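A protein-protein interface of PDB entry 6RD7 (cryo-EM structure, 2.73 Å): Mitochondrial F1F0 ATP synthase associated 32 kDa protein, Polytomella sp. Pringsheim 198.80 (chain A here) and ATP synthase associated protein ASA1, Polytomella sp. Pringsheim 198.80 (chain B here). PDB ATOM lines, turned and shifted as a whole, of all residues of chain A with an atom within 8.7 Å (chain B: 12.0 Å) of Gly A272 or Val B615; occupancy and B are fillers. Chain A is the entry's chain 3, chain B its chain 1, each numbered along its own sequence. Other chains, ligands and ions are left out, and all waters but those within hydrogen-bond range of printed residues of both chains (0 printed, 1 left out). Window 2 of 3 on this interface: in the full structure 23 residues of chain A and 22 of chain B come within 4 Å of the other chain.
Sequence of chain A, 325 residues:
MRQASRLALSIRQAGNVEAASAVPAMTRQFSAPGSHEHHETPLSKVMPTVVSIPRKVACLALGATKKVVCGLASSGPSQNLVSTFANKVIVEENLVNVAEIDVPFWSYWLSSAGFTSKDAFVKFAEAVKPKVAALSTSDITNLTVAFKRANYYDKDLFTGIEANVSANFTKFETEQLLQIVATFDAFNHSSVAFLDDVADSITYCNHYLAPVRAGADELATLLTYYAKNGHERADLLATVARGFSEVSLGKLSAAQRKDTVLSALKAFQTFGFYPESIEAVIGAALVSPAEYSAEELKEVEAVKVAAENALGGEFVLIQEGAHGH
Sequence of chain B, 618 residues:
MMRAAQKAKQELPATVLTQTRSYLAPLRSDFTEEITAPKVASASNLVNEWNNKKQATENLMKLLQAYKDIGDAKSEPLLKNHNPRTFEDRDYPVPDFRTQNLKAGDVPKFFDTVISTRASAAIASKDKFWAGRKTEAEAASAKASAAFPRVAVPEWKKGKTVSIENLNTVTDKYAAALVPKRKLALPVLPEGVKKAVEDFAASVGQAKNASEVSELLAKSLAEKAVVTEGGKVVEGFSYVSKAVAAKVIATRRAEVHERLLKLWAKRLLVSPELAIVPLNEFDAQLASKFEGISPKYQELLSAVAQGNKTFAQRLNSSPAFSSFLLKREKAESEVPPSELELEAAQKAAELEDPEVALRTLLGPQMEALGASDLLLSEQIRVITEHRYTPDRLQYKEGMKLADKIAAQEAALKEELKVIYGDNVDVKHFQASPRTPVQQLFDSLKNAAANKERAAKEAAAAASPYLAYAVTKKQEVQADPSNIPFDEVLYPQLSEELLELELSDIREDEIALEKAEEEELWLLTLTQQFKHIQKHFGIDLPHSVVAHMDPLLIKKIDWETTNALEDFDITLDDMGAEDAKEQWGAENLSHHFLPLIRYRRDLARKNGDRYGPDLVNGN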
ATOM      1  N   GLU A 232      15.205  29.143 -19.946  1.00  0.00           N
ATOM      2  CA  GLU A 232      13.810  29.289 -20.340  1.00  0.00           C
ATOM      3  C   GLU A 232      12.987  29.757 -19.150  1.00  0.00           C
ATOM      4  O   GLU A 232      12.910  29.070 -18.126  1.00  0.00           O
ATOM      5  CB  GLU A 232      13.273  27.984 -20.915  1.00  0.00           C
ATOM      6  CG  GLU A 232      11.858  28.096 -21.406  1.00  0.00           C
ATOM      7  CD  GLU A 232      11.452  26.906 -22.231  1.00  0.00           C
ATOM      8  OE1 GLU A 232      12.247  25.957 -22.353  1.00  0.00           O
ATOM      9  OE2 GLU A 232      10.346  26.934 -22.792  1.00  0.00           O
ATOM     10  N   ARG A 233      12.377  30.928 -19.294  1.00  0.00           N
ATOM     11  CA  ARG A 233      11.480  31.497 -18.301  1.00  0.00           C
ATOM     12  C   ARG A 233      10.176  31.844 -19.000  1.00  0.00           C
ATOM     13  O   ARG A 233      10.148  32.741 -19.847  1.00  0.00           O
ATOM     14  CB  ARG A 233      12.099  32.735 -17.654  1.00  0.00           C
ATOM     15  CG  ARG A 233      13.353  32.451 -16.861  1.00  0.00           C
ATOM     16  CD  ARG A 233      13.013  32.149 -15.425  1.00  0.00           C
ATOM     17  NE  ARG A 233      12.097  33.143 -14.888  1.00  0.00           N
ATOM     18  CZ  ARG A 233      12.463  34.137 -14.089  1.00  0.00           C
ATOM     19  NH1 ARG A 233      13.728  34.264 -13.731  1.00  0.00           N
ATOM     20  NH2 ARG A 233      11.560  34.999 -13.649  1.00  0.00           N
ATOM     21  N   ALA A 234       9.105  31.130 -18.650  1.00  0.00           N
ATOM     22  CA  ALA A 234       7.833  31.300 -19.345  1.00  0.00           C
ATOM     23  C   ALA A 234       7.192  32.643 -19.023  1.00  0.00           C
ATOM     24  O   ALA A 234       6.497  33.226 -19.863  1.00  0.00           O
ATOM     25  CB  ALA A 234       6.886  30.160 -18.982  1.00  0.00           C
ATOM     26  N   ASP A 235       7.424  33.152 -17.812  1.00  0.00           N
ATOM     27  CA  ASP A 235       6.874  34.445 -17.426  1.00  0.00           C
ATOM     28  C   ASP A 235       7.551  35.581 -18.183  1.00  0.00           C
ATOM     29  O   ASP A 235       6.879  36.501 -18.672  1.00  0.00           O
ATOM     30  CB  ASP A 235       7.017  34.630 -15.917  1.00  0.00           C
ATOM     31  CG  ASP A 235       8.371  34.187 -15.401  1.00  0.00           C
ATOM     32  OD1 ASP A 235       9.207  33.761 -16.218  1.00  0.00           O
ATOM     33  OD2 ASP A 235       8.601  34.258 -14.178  1.00  0.00           O
ATOM     34  N   LEU A 236       8.880  35.519 -18.304  1.00  0.00           N
ATOM     35  CA  LEU A 236       9.603  36.475 -19.133  1.00  0.00           C
ATOM     36  C   LEU A 236       9.213  36.335 -20.594  1.00  0.00           C
ATOM     37  O   LEU A 236       9.128  37.332 -21.314  1.00  0.00           O
ATOM     38  CB  LEU A 236      11.110  36.292 -18.961  1.00  0.00           C
ATOM     39  CG  LEU A 236      12.004  37.111 -19.894  1.00  0.00           C
ATOM     40  CD1 LEU A 236      12.191  38.513 -19.366  1.00  0.00           C
ATOM     41  CD2 LEU A 236      13.325  36.444 -20.122  1.00  0.00           C
ATOM     42  N   LEU A 237       8.937  35.108 -21.035  1.00  0.00           N
ATOM     43  CA  LEU A 237       8.510  34.887 -22.411  1.00  0.00           C
ATOM     44  C   LEU A 237       7.173  35.553 -22.691  1.00  0.00           C
ATOM     45  O   LEU A 237       7.008  36.193 -23.730  1.00  0.00           O
ATOM     46  CB  LEU A 237       8.434  33.393 -22.695  1.00  0.00           C
ATOM     47  CG  LEU A 237       9.776  32.831 -23.135  1.00  0.00           C
ATOM     48  CD1 LEU A 237       9.713  31.327 -23.171  1.00  0.00           C
ATOM     49  CD2 LEU A 237      10.124  33.402 -24.479  1.00  0.00           C
ATOM     50  N   ALA A 238       6.232  35.464 -21.746  1.00  0.00           N
ATOM     51  CA  ALA A 238       4.953  36.152 -21.899  1.00  0.00           C
ATOM     52  C   ALA A 238       5.122  37.668 -21.883  1.00  0.00           C
ATOM     53  O   ALA A 238       4.529  38.374 -22.712  1.00  0.00           O
ATOM     54  CB  ALA A 238       3.994  35.711 -20.797  1.00  0.00           C
ATOM     55  N   LEU A 265      10.852  34.427 -34.114  1.00  0.00           N
ATOM     56  CA  LEU A 265      10.188  33.156 -34.379  1.00  0.00           C
ATOM     57  C   LEU A 265      11.095  31.980 -34.050  1.00  0.00           C
ATOM     58  O   LEU A 265      10.621  30.948 -33.561  1.00  0.00           O
ATOM     59  CB  LEU A 265       9.731  33.091 -35.835  1.00  0.00           C
ATOM     60  CG  LEU A 265       8.521  33.945 -36.216  1.00  0.00           C
ATOM     61  CD1 LEU A 265       8.025  33.573 -37.595  1.00  0.00           C
ATOM     62  CD2 LEU A 265       7.410  33.839 -35.190  1.00  0.00           C
ATOM     63  N   LYS A 266      12.404  32.129 -34.279  1.00  0.00           N
ATOM     64  CA  LYS A 266      13.345  31.075 -33.913  1.00  0.00           C
ATOM     65  C   LYS A 266      13.417  30.893 -32.402  1.00  0.00           C
ATOM     66  O   LYS A 266      13.468  29.759 -31.913  1.00  0.00           O
ATOM     67  CB  LYS A 266      14.728  31.386 -34.479  1.00  0.00           C
ATOM     68  CG  LYS A 266      15.728  30.263 -34.296  1.00  0.00           C
ATOM     69  CD  LYS A 266      17.079  30.623 -34.879  1.00  0.00           C
ATOM     70  CE  LYS A 266      18.110  29.552 -34.570  1.00  0.00           C
ATOM     71  NZ  LYS A 266      19.452  29.909 -35.100  1.00  0.00           N
ATOM     72  N   ALA A 267      13.388  31.994 -31.645  1.00  0.00           N
ATOM     73  CA  ALA A 267      13.395  31.889 -30.187  1.00  0.00           C
ATOM     74  C   ALA A 267      12.098  31.277 -29.665  1.00  0.00           C
ATOM     75  O   ALA A 267      12.117  30.433 -28.758  1.00  0.00           O
ATOM     76  CB  ALA A 267      13.628  33.262 -29.565  1.00  0.00           C
ATOM     77  N   PHE A 268      10.960  31.685 -30.238  1.00  0.00           N
ATOM     78  CA  PHE A 268       9.670  31.153 -29.802  1.00  0.00           C
ATOM     79  C   PHE A 268       9.527  29.677 -30.152  1.00  0.00           C
ATOM     80  O   PHE A 268       8.855  28.926 -29.437  1.00  0.00           O
ATOM     81  CB  PHE A 268       8.532  31.954 -30.430  1.00  0.00           C
ATOM     82  CG  PHE A 268       8.230  33.239 -29.722  1.00  0.00           C
ATOM     83  CD1 PHE A 268       8.249  33.307 -28.340  1.00  0.00           C
ATOM     84  CD2 PHE A 268       7.918  34.380 -30.442  1.00  0.00           C
ATOM     85  CE1 PHE A 268       7.968  34.491 -27.690  1.00  0.00           C
ATOM     86  CE2 PHE A 268       7.637  35.565 -29.799  1.00  0.00           C
ATOM     87  CZ  PHE A 268       7.662  35.620 -28.423  1.00  0.00           C
ATOM     88  N   GLN A 269      10.155  29.242 -31.246  1.00  0.00           N
ATOM     89  CA  GLN A 269      10.104  27.831 -31.608  1.00  0.00           C
ATOM     90  C   GLN A 269      11.094  27.013 -30.791  1.00  0.00           C
ATOM     91  O   GLN A 269      10.857  25.828 -30.530  1.00  0.00           O
ATOM     92  CB  GLN A 269      10.378  27.669 -33.099  1.00  0.00           C
ATOM     93  CG  GLN A 269       9.872  26.376 -33.681  1.00  0.00           C
ATOM     94  CD  GLN A 269      10.488  26.090 -35.025  1.00  0.00           C
ATOM     95  OE1 GLN A 269      11.372  26.815 -35.479  1.00  0.00           O
ATOM     96  NE2 GLN A 269      10.030  25.027 -35.673  1.00  0.00           N
ATOM     97  N   THR A 270      12.216  27.624 -30.400  1.00  0.00           N
ATOM     98  CA  THR A 270      13.164  26.965 -29.508  1.00  0.00           C
ATOM     99  C   THR A 270      12.527  26.695 -28.153  1.00  0.00           C
ATOM    100  O   THR A 270      12.636  25.590 -27.609  1.00  0.00           O
ATOM    101  CB  THR A 270      14.416  27.832 -29.353  1.00  0.00           C
ATOM    102  OG1 THR A 270      15.120  27.885 -30.597  1.00  0.00           O
ATOM    103  CG2 THR A 270      15.343  27.278 -28.290  1.00  0.00           C
ATOM    104  N   PHE A 271      11.811  27.679 -27.616  1.00  0.00           N
ATOM    105  CA  PHE A 271      11.196  27.471 -26.312  1.00  0.00           C
ATOM    106  C   PHE A 271       9.907  26.671 -26.402  1.00  0.00           C
ATOM    107  O   PHE A 271       9.471  26.095 -25.400  1.00  0.00           O
ATOM    108  CB  PHE A 271      10.940  28.810 -25.644  1.00  0.00           C
ATOM    109  CG  PHE A 271      12.185  29.523 -25.257  1.00  0.00           C
ATOM    110  CD1 PHE A 271      13.181  28.857 -24.573  1.00  0.00           C
ATOM    111  CD2 PHE A 271      12.371  30.848 -25.588  1.00  0.00           C
ATOM    112  CE1 PHE A 271      14.324  29.505 -24.201  1.00  0.00           C
ATOM    113  CE2 PHE A 271      13.518  31.501 -25.228  1.00  0.00           C
ATOM    114  CZ  PHE A 271      14.491  30.829 -24.530  1.00  0.00           C
ATOM    115  N   GLY A 272       9.290  26.604 -27.576  1.00  0.00           N
ATOM    116  CA  GLY A 272       7.991  25.974 -27.673  1.00  0.00           C
ATOM    117  C   GLY A 272       6.878  26.788 -27.068  1.00  0.00           C
ATOM    118  O   GLY A 272       5.831  26.235 -26.722  1.00  0.00           O
ATOM    119  N   PHE A 273       7.080  28.092 -26.921  1.00  0.00           N
ATOM    120  CA  PHE A 273       6.098  28.995 -26.346  1.00  0.00           C
ATOM    121  C   PHE A 273       5.425  29.760 -27.473  1.00  0.00           C
ATOM    122  O   PHE A 273       6.096  30.443 -28.250  1.00  0.00           O
ATOM    123  CB  PHE A 273       6.766  29.960 -25.367  1.00  0.00           C
ATOM    124  CG  PHE A 273       5.829  30.959 -24.762  1.00  0.00           C
ATOM    125  CD1 PHE A 273       5.917  32.298 -25.097  1.00  0.00           C
ATOM    126  CD2 PHE A 273       4.869  30.560 -23.850  1.00  0.00           C
ATOM    127  CE1 PHE A 273       5.060  33.218 -24.540  1.00  0.00           C
ATOM    128  CE2 PHE A 273       4.009  31.477 -23.289  1.00  0.00           C
ATOM    129  CZ  PHE A 273       4.106  32.807 -23.635  1.00  0.00           C
ATOM    130  N   TYR A 274       4.106  29.631 -27.569  1.00  0.00           N
ATOM    131  CA  TYR A 274       3.334  30.259 -28.637  1.00  0.00           C
ATOM    132  C   TYR A 274       2.229  31.086 -27.999  1.00  0.00           C
ATOM    133  O   TYR A 274       1.139  30.575 -27.709  1.00  0.00           O
ATOM    134  CB  TYR A 274       2.782  29.216 -29.603  1.00  0.00           C
ATOM    135  CG  TYR A 274       3.860  28.320 -30.156  1.00  0.00           C
ATOM    136  CD1 TYR A 274       4.742  28.785 -31.120  1.00  0.00           C
ATOM    137  CD2 TYR A 274       4.015  27.023 -29.694  1.00  0.00           C
ATOM    138  CE1 TYR A 274       5.738  27.974 -31.619  1.00  0.00           C
ATOM    139  CE2 TYR A 274       5.004  26.206 -30.187  1.00  0.00           C
ATOM    140  CZ  TYR A 274       5.864  26.687 -31.148  1.00  0.00           C
ATOM    141  OH  TYR A 274       6.853  25.874 -31.641  1.00  0.00           O
ATOM    142  N   PRO A 275       2.480  32.371 -27.760  1.00  0.00           N
ATOM    143  CA  PRO A 275       1.448  33.236 -27.183  1.00  0.00           C
ATOM    144  C   PRO A 275       0.479  33.717 -28.243  1.00  0.00           C
ATOM    145  O   PRO A 275       0.576  33.299 -29.398  1.00  0.00           O
ATOM    146  CB  PRO A 275       2.265  34.392 -26.611  1.00  0.00           C
ATOM    147  CG  PRO A 275       3.380  34.508 -27.582  1.00  0.00           C
ATOM    148  CD  PRO A 275       3.729  33.109 -28.003  1.00  0.00           C
ATOM    149  N   ILE A 278       2.253  36.096 -31.100  1.00  0.00           N
ATOM    150  CA  ILE A 278       3.000  35.525 -32.211  1.00  0.00           C
ATOM    151  C   ILE A 278       2.242  35.697 -33.525  1.00  0.00           C
ATOM    152  O   ILE A 278       2.866  35.690 -34.593  1.00  0.00           O
ATOM    153  CB  ILE A 278       3.345  34.042 -31.929  1.00  0.00           C
ATOM    154  CG1 ILE A 278       4.511  33.575 -32.792  1.00  0.00           C
ATOM    155  CG2 ILE A 278       2.180  33.126 -32.217  1.00  0.00           C
ATOM    156  CD1 ILE A 278       5.073  32.249 -32.379  1.00  0.00           C
ATOM    157  N   ALA A 306       3.009  25.204 -35.841  1.00  0.00           N
ATOM    158  CA  ALA A 306       3.140  24.918 -34.413  1.00  0.00           C
ATOM    159  C   ALA A 306       2.288  25.861 -33.564  1.00  0.00           C
ATOM    160  O   ALA A 306       1.652  25.431 -32.594  1.00  0.00           O
ATOM    161  CB  ALA A 306       4.607  25.001 -34.003  1.00  0.00           C
ATOM    162  N   ALA A 307       2.235  27.142 -33.937  1.00  0.00           N
ATOM    163  CA  ALA A 307       1.414  28.099 -33.203  1.00  0.00           C
ATOM    164  C   ALA A 307      -0.070  27.894 -33.467  1.00  0.00           C
ATOM    165  O   ALA A 307      -0.898  28.222 -32.612  1.00  0.00           O
ATOM    166  CB  ALA A 307       1.822  29.524 -33.564  1.00  0.00           C
ATOM    167  N   ALA A 310      -0.849  25.058 -31.092  1.00  0.00           N
ATOM    168  CA  ALA A 310      -0.781  25.429 -29.681  1.00  0.00           C
ATOM    169  C   ALA A 310      -1.945  26.326 -29.276  1.00  0.00           C
ATOM    170  O   ALA A 310      -2.491  26.184 -28.177  1.00  0.00           O
ATOM    171  CB  ALA A 310       0.546  26.119 -29.383  1.00  0.00           C
ATOM    172  N   ARG B 600      12.571  28.998  -6.428  1.00  0.00           N
ATOM    173  CA  ARG B 600      13.474  28.673  -7.524  1.00  0.00           C
ATOM    174  C   ARG B 600      14.850  28.285  -7.002  1.00  0.00           C
ATOM    175  O   ARG B 600      15.483  27.367  -7.533  1.00  0.00           O
ATOM    176  CB  ARG B 600      13.576  29.849  -8.492  1.00  0.00           C
ATOM    177  CG  ARG B 600      14.392  29.548  -9.732  1.00  0.00           C
ATOM    178  CD  ARG B 600      14.598  30.774 -10.587  1.00  0.00           C
ATOM    179  NE  ARG B 600      13.363  31.513 -10.815  1.00  0.00           N
ATOM    180  CZ  ARG B 600      13.240  32.823 -10.635  1.00  0.00           C
ATOM    181  NH1 ARG B 600      14.276  33.534 -10.218  1.00  0.00           N
ATOM    182  NH2 ARG B 600      12.086  33.420 -10.871  1.00  0.00           N
ATOM    183  N   ARG B 609      14.052  21.724 -11.751  1.00  0.00           N
ATOM    184  CA  ARG B 609      13.669  22.949 -12.429  1.00  0.00           C
ATOM    185  C   ARG B 609      12.398  23.480 -11.786  1.00  0.00           C
ATOM    186  O   ARG B 609      11.527  22.703 -11.384  1.00  0.00           O
ATOM    187  CB  ARG B 609      13.447  22.710 -13.921  1.00  0.00           C
ATOM    188  CG  ARG B 609      14.707  22.357 -14.680  1.00  0.00           C
ATOM    189  CD  ARG B 609      14.382  21.815 -16.055  1.00  0.00           C
ATOM    190  NE  ARG B 609      14.684  22.784 -17.102  1.00  0.00           N
ATOM    191  CZ  ARG B 609      14.040  22.853 -18.261  1.00  0.00           C
ATOM    192  NH1 ARG B 609      14.381  23.769 -19.158  1.00  0.00           N
ATOM    193  NH2 ARG B 609      13.053  22.008 -18.524  1.00  0.00           N
ATOM    194  N   TYR B 610      12.305  24.800 -11.674  1.00  0.00           N
ATOM    195  CA  TYR B 610      11.136  25.406 -11.056  1.00  0.00           C
ATOM    196  C   TYR B 610       9.939  25.295 -11.989  1.00  0.00           C
ATOM    197  O   TYR B 610      10.040  25.587 -13.183  1.00  0.00           O
ATOM    198  CB  TYR B 610      11.420  26.864 -10.705  1.00  0.00           C
ATOM    199  CG  TYR B 610      10.343  27.511  -9.869  1.00  0.00           C
ATOM    200  CD1 TYR B 610       9.765  26.836  -8.804  1.00  0.00           C
ATOM    201  CD2 TYR B 610       9.906  28.798 -10.145  1.00  0.00           C
ATOM    202  CE1 TYR B 610       8.780  27.423  -8.041  1.00  0.00           C
ATOM    203  CE2 TYR B 610       8.922  29.394  -9.387  1.00  0.00           C
ATOM    204  CZ  TYR B 610       8.364  28.703  -8.337  1.00  0.00           C
ATOM    205  OH  TYR B 610       7.381  29.298  -7.582  1.00  0.00           O
ATOM    206  N   GLY B 611       8.816  24.846 -11.435  1.00  0.00           N
ATOM    207  CA  GLY B 611       7.596  24.600 -12.174  1.00  0.00           C
ATOM    208  C   GLY B 611       7.016  25.788 -12.920  1.00  0.00           C
ATOM    209  O   GLY B 611       6.815  25.728 -14.136  1.00  0.00           O
ATOM    210  N   PRO B 612       6.721  26.896 -12.211  1.00  0.00           N
ATOM    211  CA  PRO B 612       6.222  28.098 -12.898  1.00  0.00           C
ATOM    212  C   PRO B 612       7.199  28.788 -13.845  1.00  0.00           C
ATOM    213  O   PRO B 612       6.805  29.721 -14.549  1.00  0.00           O
ATOM    214  CB  PRO B 612       5.853  29.020 -11.732  1.00  0.00           C
ATOM    215  CG  PRO B 612       5.459  28.090 -10.662  1.00  0.00           C
ATOM    216  CD  PRO B 612       6.407  26.942 -10.770  1.00  0.00           C
ATOM    217  N   ASP B 613       8.461  28.365 -13.879  1.00  0.00           N
ATOM    218  CA  ASP B 613       9.410  28.854 -14.868  1.00  0.00           C
ATOM    219  C   ASP B 613       9.283  28.167 -16.216  1.00  0.00           C
ATOM    220  O   ASP B 613       9.658  28.755 -17.231  1.00  0.00           O
ATOM    221  CB  ASP B 613      10.847  28.678 -14.366  1.00  0.00           C
ATOM    222  CG  ASP B 613      11.256  29.745 -13.376  1.00  0.00           C
ATOM    223  OD1 ASP B 613      12.461  29.833 -13.066  1.00  0.00           O
ATOM    224  OD2 ASP B 613      10.377  30.493 -12.906  1.00  0.00           O
ATOM    225  N   LEU B 614       8.763  26.944 -16.250  1.00  0.00           N
ATOM    226  CA  LEU B 614       8.673  26.193 -17.492  1.00  0.00           C
ATOM    227  C   LEU B 614       7.402  26.552 -18.249  1.00  0.00           C
ATOM    228  O   LEU B 614       6.410  26.999 -17.669  1.00  0.00           O
ATOM    229  CB  LEU B 614       8.706  24.693 -17.207  1.00  0.00           C
ATOM    230  CG  LEU B 614       9.810  24.214 -16.264  1.00  0.00           C
ATOM    231  CD1 LEU B 614       9.672  22.730 -15.978  1.00  0.00           C
ATOM    232  CD2 LEU B 614      11.183  24.526 -16.829  1.00  0.00           C
ATOM    233  N   VAL B 615       7.441  26.346 -19.567  1.00  0.00           N
ATOM    234  CA  VAL B 615       6.297  26.675 -20.413  1.00  0.00           C
ATOM    235  C   VAL B 615       5.163  25.682 -20.208  1.00  0.00           C
ATOM    236  O   VAL B 615       4.011  26.073 -19.985  1.00  0.00           O
ATOM    237  CB  VAL B 615       6.735  26.760 -21.886  1.00  0.00           C
ATOM    238  CG1 VAL B 615       5.550  26.663 -22.818  1.00  0.00           C
ATOM    239  CG2 VAL B 615       7.403  28.081 -22.116  1.00  0.00           C
ATOM    240  N   ASN B 616       5.462  24.389 -20.259  1.00  0.00           N
ATOM    241  CA  ASN B 616       4.421  23.386 -20.102  1.00  0.00           C
ATOM    242  C   ASN B 616       4.113  23.069 -18.647  1.00  0.00           C
ATOM    243  O   ASN B 616       3.165  22.322 -18.379  1.00  0.00           O
ATOM    244  CB  ASN B 616       4.808  22.099 -20.834  1.00  0.00           C
ATOM    245  CG  ASN B 616       5.197  22.347 -22.277  1.00  0.00           C
ATOM    246  OD1 ASN B 616       6.349  22.149 -22.662  1.00  0.00           O
ATOM    247  ND2 ASN B 616       4.239  22.787 -23.082  1.00  0.00           N
ATOM    248  N   GLY B 617       4.880  23.613 -17.708  1.00  0.00           N
ATOM    249  CA  GLY B 617       4.622  23.407 -16.294  1.00  0.00           C
ATOM    250  C   GLY B 617       3.395  24.148 -15.798  1.00  0.00           C
ATOM    251  O   GLY B 617       3.498  25.086 -15.008  1.00  0.00           O
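OD2 of Asp B613 is in salt-bridge range of NE of Arg A233 (3.7 Å).
N of Ala A234 is in hydrogen-bond range of O of Asp B613.
The backbone carbonyl oxygen (O) of Asp B613 sits close to the backbone carbonyl oxygen (O) of Glu A232 (3.4 Å).
The guanidinium group of Arg B600 sits close to the guanidinium group of Arg A233.
The guanidinium group of Arg B600 lies within salt-bridge range of the side-chain carboxylate of Asp B613 (3.0 Å).
NH2 of Arg A233 lies within salt-bridge range of OD2 of Asp A235.
The backbone carbonyl oxygen of Phe A268 lies within hydrogen-bond range of the backbone NH of Phe A273 (3.2 Å).
Among the printed residues, merely in contact across the chains: Glu A232 with Val B615, Ala A234 with Leu B614, Ala A234 with Val B615, Gly A272 with Val B615 and Phe A273 with Val B615.
Gly A272 touches just one residue of chain B: Val B615.
Val B615 touches four residues of chain A.
Of the printed residues of chain B, Ala A234 touches Asp B613 (2.8 Å), Leu B614 (3.5 Å) and Val B615 (3.8 Å).
No residue of chain B comes within 4 Å of Thr A270.
No residue of chain B comes within 4 Å of Phe A271.
No residue of chain B comes within 4 Å of Tyr A274.
No residue of chain A comes within 4 Å of Asn B616.
Of the printed residues of chain B, Glu A232 touches Asp B613 (3.4 Å) and Val B615 (3.2 Å).
Printed residues of chain A within 4 Å of Asp B613: Glu A232 (3.4 Å), Arg A233 (3.4 Å) and Ala A234 (2.8 Å).
Printed residues of chain B within 4 Å of Arg A233: Arg B600 and Asp B613.
Gly B617 touches none of the printed residues of chain A.
Ala A306 touches none of the printed residues of chain B.
The nearest residue of chain B that does not touch Gly A272 is Asn B616 (5.3 Å).
The nearest printed residue of chain A that does not touch Leu B614 is Glu A232 (5.0 Å).
Of the 22 printed residues of chain A, 5 touch a printed residue of chain B.
Hydrophobic or aromatic side chains of chain A within 4 Å of the printed part of chain B: Ala A234 and Phe A273.
Among the printed residues, 9 pairs touch across the chains.
Among the printed residues, Asp or Glu carboxylates within 4 Å of a Lys or Arg side-chain nitrogen of the other chain: Arg A233 with Asp B613.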
